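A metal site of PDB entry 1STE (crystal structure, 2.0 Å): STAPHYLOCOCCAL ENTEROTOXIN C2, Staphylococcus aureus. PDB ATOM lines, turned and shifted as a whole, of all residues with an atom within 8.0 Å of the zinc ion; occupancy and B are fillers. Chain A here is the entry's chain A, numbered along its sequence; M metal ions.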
ATOM      1  N   ALA A  35      16.634 -11.088  -6.347  1.00  0.00           N
ATOM      2  CA  ALA A  35      15.745 -12.145  -6.825  1.00  0.00           C
ATOM      3  C   ALA A  35      15.900 -13.363  -5.947  1.00  0.00           C
ATOM      4  O   ALA A  35      16.983 -13.626  -5.424  1.00  0.00           O
ATOM      5  CB  ALA A  35      16.041 -12.509  -8.267  1.00  0.00           C
ATOM      6  N   THR A  36      14.824 -14.120  -5.827  1.00  0.00           N
ATOM      7  CA  THR A  36      14.801 -15.291  -4.962  1.00  0.00           C
ATOM      8  C   THR A  36      14.333 -16.545  -5.692  1.00  0.00           C
ATOM      9  O   THR A  36      13.323 -16.513  -6.380  1.00  0.00           O
ATOM     10  CB  THR A  36      13.860 -15.042  -3.759  1.00  0.00           C
ATOM     11  OG1 THR A  36      14.475 -14.094  -2.878  1.00  0.00           O
ATOM     12  CG2 THR A  36      13.607 -16.325  -2.982  1.00  0.00           C
ATOM     13  N   LYS A  37      15.124 -17.608  -5.575  1.00  0.00           N
ATOM     14  CA  LYS A  37      14.795 -18.903  -6.154  1.00  0.00           C
ATOM     15  C   LYS A  37      14.520 -18.868  -7.647  1.00  0.00           C
ATOM     16  O   LYS A  37      13.479 -19.338  -8.096  1.00  0.00           O
ATOM     17  CB  LYS A  37      13.587 -19.503  -5.432  1.00  0.00           C
ATOM     18  CG  LYS A  37      13.824 -19.731  -3.965  1.00  0.00           C
ATOM     19  CD  LYS A  37      12.525 -19.804  -3.182  1.00  0.00           C
ATOM     20  CE  LYS A  37      11.614 -20.900  -3.710  1.00  0.00           C
ATOM     21  NZ  LYS A  37      12.286 -22.226  -3.713  1.00  0.00           N
ATOM     22  N   VAL A  38      15.446 -18.309  -8.404  1.00  0.00           N
ATOM     23  CA  VAL A  38      15.292 -18.248  -9.844  1.00  0.00           C
ATOM     24  C   VAL A  38      16.291 -19.189 -10.483  1.00  0.00           C
ATOM     25  O   VAL A  38      17.226 -19.645  -9.828  1.00  0.00           O
ATOM     26  CB  VAL A  38      15.505 -16.793 -10.383  1.00  0.00           C
ATOM     27  CG1 VAL A  38      14.351 -15.902  -9.931  1.00  0.00           C
ATOM     28  CG2 VAL A  38      16.825 -16.233  -9.899  1.00  0.00           C
ATOM     29  N   VAL A  81      19.064 -23.476  -8.662  1.00  0.00           N
ATOM     30  CA  VAL A  81      18.050 -22.566  -8.142  1.00  0.00           C
ATOM     31  C   VAL A  81      18.824 -21.590  -7.250  1.00  0.00           C
ATOM     32  O   VAL A  81      19.333 -21.987  -6.203  1.00  0.00           O
ATOM     33  CB  VAL A  81      16.984 -23.314  -7.330  1.00  0.00           C
ATOM     34  CG1 VAL A  81      16.004 -22.326  -6.700  1.00  0.00           C
ATOM     35  CG2 VAL A  81      16.264 -24.270  -8.249  1.00  0.00           C
ATOM     36  N   VAL A  82      18.939 -20.346  -7.678  1.00  0.00           N
ATOM     37  CA  VAL A  82      19.724 -19.359  -6.956  1.00  0.00           C
ATOM     38  C   VAL A  82      18.997 -18.117  -6.467  1.00  0.00           C
ATOM     39  O   VAL A  82      17.830 -17.870  -6.790  1.00  0.00           O
ATOM     40  CB  VAL A  82      20.899 -18.879  -7.846  1.00  0.00           C
ATOM     41  CG1 VAL A  82      21.742 -20.071  -8.305  1.00  0.00           C
ATOM     42  CG2 VAL A  82      20.371 -18.137  -9.052  1.00  0.00           C
ATOM     43  N   ASP A  83      19.704 -17.356  -5.636  1.00  0.00           N
ATOM     44  CA  ASP A  83      19.216 -16.083  -5.131  1.00  0.00           C
ATOM     45  C   ASP A  83      20.187 -15.111  -5.788  1.00  0.00           C
ATOM     46  O   ASP A  83      21.365 -15.441  -5.998  1.00  0.00           O
ATOM     47  CB  ASP A  83      19.337 -15.995  -3.608  1.00  0.00           C
ATOM     48  CG  ASP A  83      18.300 -16.848  -2.889  1.00  0.00           C
ATOM     49  OD1 ASP A  83      17.226 -17.151  -3.473  1.00  0.00           O
ATOM     50  OD2 ASP A  83      18.555 -17.205  -1.726  1.00  0.00           O
ATOM     51  N   VAL A  84      19.694 -13.932  -6.145  1.00  0.00           N
ATOM     52  CA  VAL A  84      20.501 -12.919  -6.822  1.00  0.00           C
ATOM     53  C   VAL A  84      20.474 -11.590  -6.065  1.00  0.00           C
ATOM     54  O   VAL A  84      19.460 -11.211  -5.479  1.00  0.00           O
ATOM     55  CB  VAL A  84      19.961 -12.656  -8.273  1.00  0.00           C
ATOM     56  CG1 VAL A  84      20.863 -11.670  -9.019  1.00  0.00           C
ATOM     57  CG2 VAL A  84      19.852 -13.955  -9.055  1.00  0.00           C
ATOM     58  N   THR A 116      24.077 -16.846  -5.489  1.00  0.00           N
ATOM     59  CA  THR A 116      24.309 -17.794  -4.376  1.00  0.00           C
ATOM     60  C   THR A 116      23.214 -18.861  -4.413  1.00  0.00           C
ATOM     61  O   THR A 116      22.040 -18.557  -4.665  1.00  0.00           O
ATOM     62  CB  THR A 116      24.308 -17.135  -2.969  1.00  0.00           C
ATOM     63  OG1 THR A 116      23.153 -16.308  -2.797  1.00  0.00           O
ATOM     64  CG2 THR A 116      25.544 -16.313  -2.754  1.00  0.00           C
ATOM     65  N   LYS A 117      23.578 -20.117  -4.174  1.00  0.00           N
ATOM     66  CA  LYS A 117      22.584 -21.189  -4.169  1.00  0.00           C
ATOM     67  C   LYS A 117      21.569 -20.902  -3.077  1.00  0.00           C
ATOM     68  O   LYS A 117      21.918 -20.422  -2.002  1.00  0.00           O
ATOM     69  CB  LYS A 117      23.233 -22.534  -3.900  1.00  0.00           C
ATOM     70  CG  LYS A 117      23.768 -23.230  -5.128  1.00  0.00           C
ATOM     71  CD  LYS A 117      24.223 -24.633  -4.760  1.00  0.00           C
ATOM     72  CE  LYS A 117      23.175 -25.355  -3.893  1.00  0.00           C
ATOM     73  NZ  LYS A 117      23.638 -26.690  -3.401  1.00  0.00           N
ATOM     74  N   HIS A 118      20.299 -21.158  -3.377  1.00  0.00           N
ATOM     75  CA  HIS A 118      19.227 -20.918  -2.434  1.00  0.00           C
ATOM     76  C   HIS A 118      19.173 -21.986  -1.354  1.00  0.00           C
ATOM     77  O   HIS A 118      19.149 -21.675  -0.175  1.00  0.00           O
ATOM     78  CB  HIS A 118      17.860 -20.830  -3.152  1.00  0.00           C
ATOM     79  CG  HIS A 118      16.682 -20.979  -2.237  1.00  0.00           C
ATOM     80  ND1 HIS A 118      16.121 -19.919  -1.553  1.00  0.00           N
ATOM     81  CD2 HIS A 118      15.983 -22.074  -1.856  1.00  0.00           C
ATOM     82  CE1 HIS A 118      15.160 -20.361  -0.774  1.00  0.00           C
ATOM     83  NE2 HIS A 118      15.051 -21.656  -0.940  1.00  0.00           N
ATOM     84  N   GLU A 119      19.086 -23.234  -1.782  1.00  0.00           N
ATOM     85  CA  GLU A 119      18.980 -24.356  -0.847  1.00  0.00           C
ATOM     86  C   GLU A 119      20.099 -24.471   0.152  1.00  0.00           C
ATOM     87  O   GLU A 119      21.277 -24.483  -0.193  1.00  0.00           O
ATOM     88  CB  GLU A 119      18.795 -25.672  -1.593  1.00  0.00           C
ATOM     89  CG  GLU A 119      17.368 -25.868  -2.087  1.00  0.00           C
ATOM     90  CD  GLU A 119      17.182 -27.124  -2.915  1.00  0.00           C
ATOM     91  OE1 GLU A 119      17.519 -28.223  -2.409  1.00  0.00           O
ATOM     92  OE2 GLU A 119      16.707 -27.016  -4.070  1.00  0.00           O
ATOM     93  N   GLY A 120      19.703 -24.465   1.419  1.00  0.00           N
ATOM     94  CA  GLY A 120      20.654 -24.603   2.504  1.00  0.00           C
ATOM     95  C   GLY A 120      21.499 -23.392   2.808  1.00  0.00           C
ATOM     96  O   GLY A 120      22.384 -23.469   3.639  1.00  0.00           O
ATOM     97  N   ASN A 121      21.190 -22.251   2.196  1.00  0.00           N
ATOM     98  CA  ASN A 121      21.981 -21.053   2.414  1.00  0.00           C
ATOM     99  C   ASN A 121      21.355 -20.064   3.369  1.00  0.00           C
ATOM    100  O   ASN A 121      21.779 -18.914   3.438  1.00  0.00           O
ATOM    101  CB  ASN A 121      22.246 -20.349   1.087  1.00  0.00           C
ATOM    102  CG  ASN A 121      23.383 -19.364   1.165  1.00  0.00           C
ATOM    103  OD1 ASN A 121      23.337 -18.277   0.576  1.00  0.00           O
ATOM    104  ND2 ASN A 121      24.406 -19.731   1.886  1.00  0.00           N
ATOM    105  N   HIS A 122      20.327 -20.482   4.099  1.00  0.00           N
ATOM    106  CA  HIS A 122      19.637 -19.576   5.020  1.00  0.00           C
ATOM    107  C   HIS A 122      19.687 -20.014   6.481  1.00  0.00           C
ATOM    108  O   HIS A 122      19.882 -21.195   6.772  1.00  0.00           O
ATOM    109  CB  HIS A 122      18.198 -19.323   4.540  1.00  0.00           C
ATOM    110  CG  HIS A 122      18.130 -18.565   3.251  1.00  0.00           C
ATOM    111  ND1 HIS A 122      18.402 -17.219   3.186  1.00  0.00           N
ATOM    112  CD2 HIS A 122      17.965 -18.981   1.974  1.00  0.00           C
ATOM    113  CE1 HIS A 122      18.424 -16.832   1.919  1.00  0.00           C
ATOM    114  NE2 HIS A 122      18.167 -17.891   1.160  1.00  0.00           N
ATOM    115  N   ASP A 150      20.464 -12.401   5.020  1.00  0.00           N
ATOM    116  CA  ASP A 150      19.824 -13.638   5.427  1.00  0.00           C
ATOM    117  C   ASP A 150      20.566 -14.835   4.830  1.00  0.00           C
ATOM    118  O   ASP A 150      20.081 -15.959   4.888  1.00  0.00           O
ATOM    119  CB  ASP A 150      18.354 -13.657   4.980  1.00  0.00           C
ATOM    120  CG  ASP A 150      18.183 -13.605   3.467  1.00  0.00           C
ATOM    121  OD1 ASP A 150      19.061 -13.099   2.740  1.00  0.00           O
ATOM    122  OD2 ASP A 150      17.134 -14.072   2.982  1.00  0.00           O
ATOM    123  N   LYS A 151      21.718 -14.582   4.229  1.00  0.00           N
ATOM    124  CA  LYS A 151      22.482 -15.651   3.630  1.00  0.00           C
ATOM    125  C   LYS A 151      23.672 -16.045   4.497  1.00  0.00           C
ATOM    126  O   LYS A 151      24.304 -15.185   5.133  1.00  0.00           O
ATOM    127  CB  LYS A 151      22.973 -15.230   2.252  1.00  0.00           C
ATOM    128  CG  LYS A 151      21.867 -14.926   1.256  1.00  0.00           C
ATOM    129  CD  LYS A 151      22.433 -14.129   0.097  1.00  0.00           C
ATOM    130  CE  LYS A 151      21.352 -13.291  -0.612  1.00  0.00           C
ATOM    131  NZ  LYS A 151      20.537 -14.159  -1.468  1.00  0.00           N
HETATM  132 ZN    ZN M   1      17.130 -18.096  -0.777  1.00  0.00          ZN
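ND1 of His 122 sits at hydrogen-bond distance from O of Asp 150 (2.7 Å).
OD2 of Asp 83 lies close to NZ of Lys 151 (3.6 Å).
The backbone NH (N) of Asp 83 is in hydrogen-bond range of the backbone carbonyl oxygen (O) of Thr 116 (2.8 Å).
The side-chain carboxylate (OD1) of Asp 83 lies within hydrogen-bond range of the backbone NH (N) of Lys 37, at 3.0 Å.
The backbone NH of His 118 is in hydrogen-bond range of the backbone carbonyl oxygen of Val 81 (3.1 Å).
The nearest printed residue that does not touch the zinc ion is Thr 36 (4.5 Å).
The zinc ion is bound by the side-chain carboxylate of Asp 83 (1.9 Å), a ring nitrogen (NE2) of His 122 (2.2 Å) and a ring nitrogen (ND1) of His 118 (2.2 Å).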
